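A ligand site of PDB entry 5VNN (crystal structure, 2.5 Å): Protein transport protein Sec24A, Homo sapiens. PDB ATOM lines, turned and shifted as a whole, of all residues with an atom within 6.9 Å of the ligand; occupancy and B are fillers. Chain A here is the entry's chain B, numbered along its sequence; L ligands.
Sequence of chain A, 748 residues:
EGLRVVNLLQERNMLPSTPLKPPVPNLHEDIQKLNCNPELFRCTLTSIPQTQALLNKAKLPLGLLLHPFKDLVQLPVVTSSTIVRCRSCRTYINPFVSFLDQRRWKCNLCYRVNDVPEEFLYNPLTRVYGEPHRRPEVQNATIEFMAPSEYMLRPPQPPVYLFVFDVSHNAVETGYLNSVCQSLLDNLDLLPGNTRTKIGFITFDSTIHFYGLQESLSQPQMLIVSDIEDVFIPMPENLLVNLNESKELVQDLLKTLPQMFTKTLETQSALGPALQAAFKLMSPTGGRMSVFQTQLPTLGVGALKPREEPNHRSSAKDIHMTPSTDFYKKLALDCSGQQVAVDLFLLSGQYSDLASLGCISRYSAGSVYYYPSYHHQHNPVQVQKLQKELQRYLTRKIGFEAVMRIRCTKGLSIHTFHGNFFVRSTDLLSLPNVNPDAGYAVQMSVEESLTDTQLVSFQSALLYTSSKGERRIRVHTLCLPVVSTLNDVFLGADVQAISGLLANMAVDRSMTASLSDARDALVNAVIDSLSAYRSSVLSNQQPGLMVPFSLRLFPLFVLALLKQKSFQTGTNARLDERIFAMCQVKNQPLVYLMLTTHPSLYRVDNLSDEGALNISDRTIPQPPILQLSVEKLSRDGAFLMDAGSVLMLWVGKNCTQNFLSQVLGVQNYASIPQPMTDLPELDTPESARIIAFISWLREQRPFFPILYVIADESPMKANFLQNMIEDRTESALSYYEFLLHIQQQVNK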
ATOM      1  N   ARG A  85      -7.990  13.624   7.358  1.00  0.00           N
ATOM      2  CA  ARG A  85      -6.547  13.825   7.342  1.00  0.00           C
ATOM      3  C   ARG A  85      -6.144  14.619   8.567  1.00  0.00           C
ATOM      4  O   ARG A  85      -6.813  15.586   8.933  1.00  0.00           O
ATOM      5  CB  ARG A  85      -6.097  14.546   6.067  1.00  0.00           C
ATOM      6  CG  ARG A  85      -6.531  13.872   4.785  1.00  0.00           C
ATOM      7  CD  ARG A  85      -6.003  14.611   3.574  1.00  0.00           C
ATOM      8  NE  ARG A  85      -4.547  14.513   3.464  1.00  0.00           N
ATOM      9  CZ  ARG A  85      -3.837  15.048   2.484  1.00  0.00           C
ATOM     10  NH1 ARG A  85      -4.446  15.726   1.511  1.00  0.00           N
ATOM     11  NH2 ARG A  85      -2.520  14.922   2.460  1.00  0.00           N
ATOM     12  N   CYS A  89       0.103  17.300   9.803  1.00  0.00           N
ATOM     13  CA  CYS A  89       0.946  16.711   8.778  1.00  0.00           C
ATOM     14  C   CYS A  89       0.158  16.121   7.609  1.00  0.00           C
ATOM     15  O   CYS A  89       0.775  15.577   6.678  1.00  0.00           O
ATOM     16  CB  CYS A  89       1.843  15.623   9.374  1.00  0.00           C
ATOM     17  SG  CYS A  89       0.940  14.134   9.857  1.00  0.00           S
ATOM     18  N   ARG A  90      -1.163  16.211   7.640  1.00  0.00           N
ATOM     19  CA  ARG A  90      -2.056  15.758   6.565  1.00  0.00           C
ATOM     20  C   ARG A  90      -2.002  14.255   6.337  1.00  0.00           C
ATOM     21  O   ARG A  90      -2.288  13.791   5.221  1.00  0.00           O
ATOM     22  CB  ARG A  90      -1.770  16.506   5.256  1.00  0.00           C
ATOM     23  CG  ARG A  90      -1.797  18.022   5.361  1.00  0.00           C
ATOM     24  CD  ARG A  90      -3.036  18.503   6.092  1.00  0.00           C
ATOM     25  NE  ARG A  90      -4.265  17.944   5.544  1.00  0.00           N
ATOM     26  CZ  ARG A  90      -5.002  18.507   4.591  1.00  0.00           C
ATOM     27  NH1 ARG A  90      -4.633  19.679   4.078  1.00  0.00           N
ATOM     28  NH2 ARG A  90      -6.101  17.914   4.153  1.00  0.00           N
ATOM     29  N   TYR A  92      -3.340  10.584   6.246  1.00  0.00           N
ATOM     30  CA  TYR A  92      -4.677  10.013   6.114  1.00  0.00           C
ATOM     31  C   TYR A  92      -4.968   9.054   7.262  1.00  0.00           C
ATOM     32  O   TYR A  92      -4.065   8.407   7.806  1.00  0.00           O
ATOM     33  CB  TYR A  92      -4.807   9.292   4.780  1.00  0.00           C
ATOM     34  CG  TYR A  92      -4.779  10.231   3.594  1.00  0.00           C
ATOM     35  CD1 TYR A  92      -3.578  10.705   3.074  1.00  0.00           C
ATOM     36  CD2 TYR A  92      -5.963  10.651   2.995  1.00  0.00           C
ATOM     37  CE1 TYR A  92      -3.556  11.566   1.991  1.00  0.00           C
ATOM     38  CE2 TYR A  92      -5.949  11.508   1.916  1.00  0.00           C
ATOM     39  CZ  TYR A  92      -4.741  11.958   1.416  1.00  0.00           C
ATOM     40  OH  TYR A  92      -4.749  12.816   0.340  1.00  0.00           O
ATOM     41  N   ALA A 147     -10.797  11.753  -4.660  1.00  0.00           N
ATOM     42  CA  ALA A 147     -10.280  13.069  -4.321  1.00  0.00           C
ATOM     43  C   ALA A 147     -11.339  14.140  -4.609  1.00  0.00           C
ATOM     44  O   ALA A 147     -11.931  14.136  -5.687  1.00  0.00           O
ATOM     45  CB  ALA A 147      -9.013  13.363  -5.109  1.00  0.00           C
ATOM     46  N   TYR A 151      -8.348  18.730  -4.726  1.00  0.00           N
ATOM     47  CA  TYR A 151      -7.150  17.956  -4.952  1.00  0.00           C
ATOM     48  C   TYR A 151      -6.763  17.905  -6.431  1.00  0.00           C
ATOM     49  O   TYR A 151      -5.919  17.083  -6.809  1.00  0.00           O
ATOM     50  CB  TYR A 151      -7.328  16.529  -4.422  1.00  0.00           C
ATOM     51  CG  TYR A 151      -7.331  16.427  -2.910  1.00  0.00           C
ATOM     52  CD1 TYR A 151      -8.243  17.143  -2.149  1.00  0.00           C
ATOM     53  CD2 TYR A 151      -6.448  15.592  -2.245  1.00  0.00           C
ATOM     54  CE1 TYR A 151      -8.262  17.060  -0.775  1.00  0.00           C
ATOM     55  CE2 TYR A 151      -6.464  15.476  -0.868  1.00  0.00           C
ATOM     56  CZ  TYR A 151      -7.368  16.220  -0.144  1.00  0.00           C
ATOM     57  OH  TYR A 151      -7.396  16.133   1.233  1.00  0.00           O
ATOM     58  N   VAL A 403       0.971  12.807  -8.391  1.00  0.00           N
ATOM     59  CA  VAL A 403       2.034  13.099  -7.447  1.00  0.00           C
ATOM     60  C   VAL A 403       1.947  12.084  -6.316  1.00  0.00           C
ATOM     61  O   VAL A 403       0.899  11.489  -6.074  1.00  0.00           O
ATOM     62  CB  VAL A 403       1.972  14.547  -6.893  1.00  0.00           C
ATOM     63  CG1 VAL A 403       1.690  15.549  -7.998  1.00  0.00           C
ATOM     64  CG2 VAL A 403       0.945  14.643  -5.770  1.00  0.00           C
ATOM     65  N   MET A 404       3.076  11.886  -5.637  1.00  0.00           N
ATOM     66  CA  MET A 404       3.147  10.924  -4.551  1.00  0.00           C
ATOM     67  C   MET A 404       3.941  11.513  -3.394  1.00  0.00           C
ATOM     68  O   MET A 404       4.952  12.192  -3.609  1.00  0.00           O
ATOM     69  CB  MET A 404       3.780   9.599  -4.997  1.00  0.00           C
ATOM     70  CG  MET A 404       3.700   8.487  -3.959  1.00  0.00           C
ATOM     71  SD  MET A 404       4.246   6.888  -4.579  1.00  0.00           S
ATOM     72  CE  MET A 404       5.957   7.233  -4.957  1.00  0.00           C
ATOM     73  N   ARG A 405       3.468  11.263  -2.176  1.00  0.00           N
ATOM     74  CA  ARG A 405       4.097  11.731  -0.954  1.00  0.00           C
ATOM     75  C   ARG A 405       4.427  10.529  -0.071  1.00  0.00           C
ATOM     76  O   ARG A 405       3.584   9.645   0.101  1.00  0.00           O
ATOM     77  CB  ARG A 405       3.201  12.715  -0.204  1.00  0.00           C
ATOM     78  CG  ARG A 405       3.747  13.206   1.124  1.00  0.00           C
ATOM     79  CD  ARG A 405       4.380  14.566   0.986  1.00  0.00           C
ATOM     80  NE  ARG A 405       3.417  15.586   0.590  1.00  0.00           N
ATOM     81  CZ  ARG A 405       3.729  16.828   0.247  1.00  0.00           C
ATOM     82  NH1 ARG A 405       4.997  17.219   0.239  1.00  0.00           N
ATOM     83  NH2 ARG A 405       2.775  17.688  -0.103  1.00  0.00           N
ATOM     84  N   ARG A 407       5.313   9.646   3.670  1.00  0.00           N
ATOM     85  CA  ARG A 407       5.297  10.147   5.031  1.00  0.00           C
ATOM     86  C   ARG A 407       5.774   9.082   6.002  1.00  0.00           C
ATOM     87  O   ARG A 407       5.455   7.901   5.842  1.00  0.00           O
ATOM     88  CB  ARG A 407       3.903  10.624   5.428  1.00  0.00           C
ATOM     89  CG  ARG A 407       3.425  11.887   4.737  1.00  0.00           C
ATOM     90  CD  ARG A 407       2.146  12.399   5.373  1.00  0.00           C
ATOM     91  NE  ARG A 407       1.613  13.566   4.669  1.00  0.00           N
ATOM     92  CZ  ARG A 407       0.735  13.497   3.678  1.00  0.00           C
ATOM     93  NH1 ARG A 407       0.282  12.314   3.268  1.00  0.00           N
ATOM     94  NH2 ARG A 407       0.312  14.598   3.091  1.00  0.00           N
ATOM     95  N   ASP A 427       9.940  15.242  -0.212  1.00  0.00           N
ATOM     96  CA  ASP A 427       8.682  14.516  -0.114  1.00  0.00           C
ATOM     97  C   ASP A 427       7.610  15.195  -0.960  1.00  0.00           C
ATOM     98  O   ASP A 427       6.738  15.891  -0.444  1.00  0.00           O
ATOM     99  CB  ASP A 427       8.222  14.398   1.343  1.00  0.00           C
ATOM    100  CG  ASP A 427       8.796  13.176   2.030  1.00  0.00           C
ATOM    101  OD1 ASP A 427       8.955  12.147   1.339  1.00  0.00           O
ATOM    102  OD2 ASP A 427       9.056  13.240   3.249  1.00  0.00           O
ATOM    103  N   LEU A 428       7.841  15.185  -2.259  1.00  0.00           N
ATOM    104  CA  LEU A 428       6.843  15.553  -3.239  1.00  0.00           C
ATOM    105  C   LEU A 428       7.259  15.013  -4.576  1.00  0.00           C
ATOM    106  O   LEU A 428       8.052  15.588  -5.246  1.00  0.00           O
ATOM    107  CB  LEU A 428       6.461  16.987  -3.236  1.00  0.00           C
ATOM    108  CG  LEU A 428       5.068  17.030  -3.815  1.00  0.00           C
ATOM    109  CD1 LEU A 428       4.233  15.866  -3.411  1.00  0.00           C
ATOM    110  CD2 LEU A 428       4.372  18.288  -3.426  1.00  0.00           C
ATOM    111  N   GLN A 459       3.627   6.098   5.585  1.00  0.00           N
ATOM    112  CA  GLN A 459       2.481   6.257   4.704  1.00  0.00           C
ATOM    113  C   GLN A 459       2.933   6.816   3.366  1.00  0.00           C
ATOM    114  O   GLN A 459       3.670   7.808   3.313  1.00  0.00           O
ATOM    115  CB  GLN A 459       1.420   7.175   5.317  1.00  0.00           C
ATOM    116  CG  GLN A 459       0.107   7.171   4.565  1.00  0.00           C
ATOM    117  CD  GLN A 459      -0.781   8.330   4.947  1.00  0.00           C
ATOM    118  OE1 GLN A 459      -1.886   8.138   5.468  1.00  0.00           O
ATOM    119  NE2 GLN A 459      -0.317   9.542   4.687  1.00  0.00           N
ATOM    120  N   SER A 460       2.481   6.185   2.291  1.00  0.00           N
ATOM    121  CA  SER A 460       2.593   6.714   0.947  1.00  0.00           C
ATOM    122  C   SER A 460       1.199   6.823   0.350  1.00  0.00           C
ATOM    123  O   SER A 460       0.310   6.021   0.673  1.00  0.00           O
ATOM    124  CB  SER A 460       3.479   5.833   0.053  1.00  0.00           C
ATOM    125  OG  SER A 460       2.759   4.713  -0.430  1.00  0.00           O
ATOM    126  N   ALA A 461       0.996   7.821  -0.503  1.00  0.00           N
ATOM    127  CA  ALA A 461      -0.316   8.057  -1.073  1.00  0.00           C
ATOM    128  C   ALA A 461      -0.149   8.581  -2.493  1.00  0.00           C
ATOM    129  O   ALA A 461       0.769   9.352  -2.775  1.00  0.00           O
ATOM    130  CB  ALA A 461      -1.129   9.026  -0.221  1.00  0.00           C
ATOM    131  N   LEU A 462      -1.046   8.152  -3.377  1.00  0.00           N
ATOM    132  CA  LEU A 462      -0.920   8.383  -4.815  1.00  0.00           C
ATOM    133  C   LEU A 462      -2.155   9.143  -5.309  1.00  0.00           C
ATOM    134  O   LEU A 462      -3.205   8.551  -5.534  1.00  0.00           O
ATOM    135  CB  LEU A 462      -0.753   7.055  -5.555  1.00  0.00           C
ATOM    136  CG  LEU A 462       0.057   7.030  -6.853  1.00  0.00           C
ATOM    137  CD1 LEU A 462       0.679   8.383  -7.142  1.00  0.00           C
ATOM    138  CD2 LEU A 462       1.123   5.947  -6.762  1.00  0.00           C
ATOM    139  N   LEU A 463      -2.011  10.455  -5.470  1.00  0.00           N
ATOM    140  CA  LEU A 463      -3.043  11.282  -6.079  1.00  0.00           C
ATOM    141  C   LEU A 463      -2.881  11.235  -7.592  1.00  0.00           C
ATOM    142  O   LEU A 463      -1.868  11.707  -8.117  1.00  0.00           O
ATOM    143  CB  LEU A 463      -2.969  12.722  -5.571  1.00  0.00           C
ATOM    144  CG  LEU A 463      -3.865  13.762  -6.246  1.00  0.00           C
ATOM    145  CD1 LEU A 463      -5.329  13.422  -6.031  1.00  0.00           C
ATOM    146  CD2 LEU A 463      -3.558  15.153  -5.709  1.00  0.00           C
ATOM    147  N   TYR A 464      -3.865  10.673  -8.288  1.00  0.00           N
ATOM    148  CA  TYR A 464      -3.766  10.538  -9.738  1.00  0.00           C
ATOM    149  C   TYR A 464      -5.149  10.683 -10.353  1.00  0.00           C
ATOM    150  O   TYR A 464      -6.176  10.586  -9.678  1.00  0.00           O
ATOM    151  CB  TYR A 464      -3.155   9.184 -10.123  1.00  0.00           C
ATOM    152  CG  TYR A 464      -4.060   7.995  -9.894  1.00  0.00           C
ATOM    153  CD1 TYR A 464      -4.189   7.431  -8.630  1.00  0.00           C
ATOM    154  CD2 TYR A 464      -4.790   7.444 -10.936  1.00  0.00           C
ATOM    155  CE1 TYR A 464      -5.017   6.342  -8.416  1.00  0.00           C
ATOM    156  CE2 TYR A 464      -5.625   6.359 -10.733  1.00  0.00           C
ATOM    157  CZ  TYR A 464      -5.735   5.806  -9.468  1.00  0.00           C
ATOM    158  OH  TYR A 464      -6.559   4.729  -9.260  1.00  0.00           O
ATOM    159  N   ARG A 472      -8.371  10.082  -7.887  1.00  0.00           N
ATOM    160  CA  ARG A 472      -8.342   9.052  -6.862  1.00  0.00           C
ATOM    161  C   ARG A 472      -7.048   9.166  -6.065  1.00  0.00           C
ATOM    162  O   ARG A 472      -6.049   9.720  -6.535  1.00  0.00           O
ATOM    163  CB  ARG A 472      -8.469   7.648  -7.463  1.00  0.00           C
ATOM    164  CG  ARG A 472      -9.743   7.415  -8.257  1.00  0.00           C
ATOM    165  CD  ARG A 472     -10.249   6.001  -8.065  1.00  0.00           C
ATOM    166  NE  ARG A 472     -11.440   5.728  -8.869  1.00  0.00           N
ATOM    167  CZ  ARG A 472     -12.218   4.662  -8.709  1.00  0.00           C
ATOM    168  NH1 ARG A 472     -11.937   3.772  -7.775  1.00  0.00           N
ATOM    169  NH2 ARG A 472     -13.281   4.496  -9.485  1.00  0.00           N
ATOM    170  N   ILE A 473      -7.088   8.628  -4.842  1.00  0.00           N
ATOM    171  CA  ILE A 473      -5.947   8.627  -3.941  1.00  0.00           C
ATOM    172  C   ILE A 473      -5.796   7.217  -3.386  1.00  0.00           C
ATOM    173  O   ILE A 473      -6.635   6.774  -2.597  1.00  0.00           O
ATOM    174  CB  ILE A 473      -6.103   9.637  -2.798  1.00  0.00           C
ATOM    175  CG1 ILE A 473      -6.439  11.029  -3.341  1.00  0.00           C
ATOM    176  CG2 ILE A 473      -4.826   9.694  -1.961  1.00  0.00           C
ATOM    177  CD1 ILE A 473      -6.611  12.068  -2.263  1.00  0.00           C
ATOM    178  N   ARG A 474      -4.738   6.523  -3.785  1.00  0.00           N
ATOM    179  CA  ARG A 474      -4.427   5.193  -3.264  1.00  0.00           C
ATOM    180  C   ARG A 474      -3.388   5.342  -2.164  1.00  0.00           C
ATOM    181  O   ARG A 474      -2.290   5.862  -2.394  1.00  0.00           O
ATOM    182  CB  ARG A 474      -3.920   4.265  -4.371  1.00  0.00           C
ATOM    183  CG  ARG A 474      -3.698   2.837  -3.922  1.00  0.00           C
ATOM    184  CD  ARG A 474      -3.478   1.890  -5.095  1.00  0.00           C
ATOM    185  NE  ARG A 474      -4.645   1.834  -5.977  1.00  0.00           N
ATOM    186  CZ  ARG A 474      -4.803   0.928  -6.946  1.00  0.00           C
ATOM    187  NH1 ARG A 474      -3.874  -0.005  -7.148  1.00  0.00           N
ATOM    188  NH2 ARG A 474      -5.884   0.949  -7.702  1.00  0.00           N
ATOM    189  N   VAL A 475      -3.739   4.883  -0.957  1.00  0.00           N
ATOM    190  CA  VAL A 475      -2.940   5.104   0.238  1.00  0.00           C
ATOM    191  C   VAL A 475      -2.506   3.754   0.810  1.00  0.00           C
ATOM    192  O   VAL A 475      -3.333   2.837   0.926  1.00  0.00           O
ATOM    193  CB  VAL A 475      -3.706   5.915   1.294  1.00  0.00           C
ATOM    194  CG1 VAL A 475      -2.840   6.175   2.526  1.00  0.00           C
ATOM    195  CG2 VAL A 475      -4.209   7.219   0.701  1.00  0.00           C
HETATM  196  C1  LIG L   1      -1.676  17.018  -0.789  1.00  0.00           C
HETATM  197  C2  LIG L   1      -1.708  16.883  -2.302  1.00  0.00           C
HETATM  198  C3  LIG L   1      -0.793  15.757  -2.782  1.00  0.00           C
HETATM  199  C4  LIG L   1      -1.259  14.404  -2.248  1.00  0.00           C
HETATM  200  C5  LIG L   1      -2.545  13.984  -2.523  1.00  0.00           C
HETATM  201  C6  LIG L   1      -0.415  13.615  -1.484  1.00  0.00           C
HETATM  202  C7  LIG L   1      -2.988  12.754  -2.059  1.00  0.00           C
HETATM  203  C8  LIG L   1      -0.861  12.397  -1.013  1.00  0.00           C
HETATM  204  C9  LIG L   1      -2.149  11.972  -1.297  1.00  0.00           C
HETATM  205  C10 LIG L   1      -0.250  17.219  -0.291  1.00  0.00           C
HETATM  206  O1  LIG L   1       0.289  18.358  -0.357  1.00  0.00           O
HETATM  207  O2  LIG L   1       0.398  16.250   0.192  1.00  0.00           O
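NH2 of Arg 405 is in salt-bridge range of O1 of the ligand (2.6 Å). The guanidinium group (NH2) of Arg 407 is in salt-bridge range of an oxygen (O2) of the ligand, at 3.3 Å. The guanidinium group (NH2) of Arg 85 lies within salt-bridge range of an oxygen (O2) of the ligand, 3.9 Å away.
The backbone carbonyl oxygen (O) of Arg 405 is in hydrogen-bond range of the backbone NH (N) of Ala 461. O of Asp 427 sits close to NE of Arg 405 (3.5 Å). OH of Tyr 92 lies within hydrogen-bond range of NH1 of Arg 85 (3.2 Å). N of Val 403 lies within hydrogen-bond range of O of Leu 463 (3.1 Å). O of Arg 90 lies close to NH2 of Arg 407, at 3.5 Å. The guanidinium group (NE) of Arg 407 is in hydrogen-bond range of the backbone carbonyl oxygen (O) of Cys 89, 3.0 Å away. The guanidinium group (NH1) of Arg 85 lies within hydrogen-bond range of the side-chain hydroxyl (OH) of Tyr 151 (3.0 Å). The guanidinium group (NE) of Arg 85 is in hydrogen-bond range of the backbone carbonyl oxygen (O) of Arg 90, 3.0 Å away.
Residues that only touch the ligand: Tyr 92, Ala 461, Leu 463, Ile 473 and Val 403. Hydrophobic or aromatic side chains that line the ligand: Tyr 92, Val 403, Ala 461, Leu 463 and Ile 473. Along chain A the residues within 4 Å of the ligand span positions 85 to 473. The nearest printed residue that does not touch the ligand is Tyr 151 (4.2 Å).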
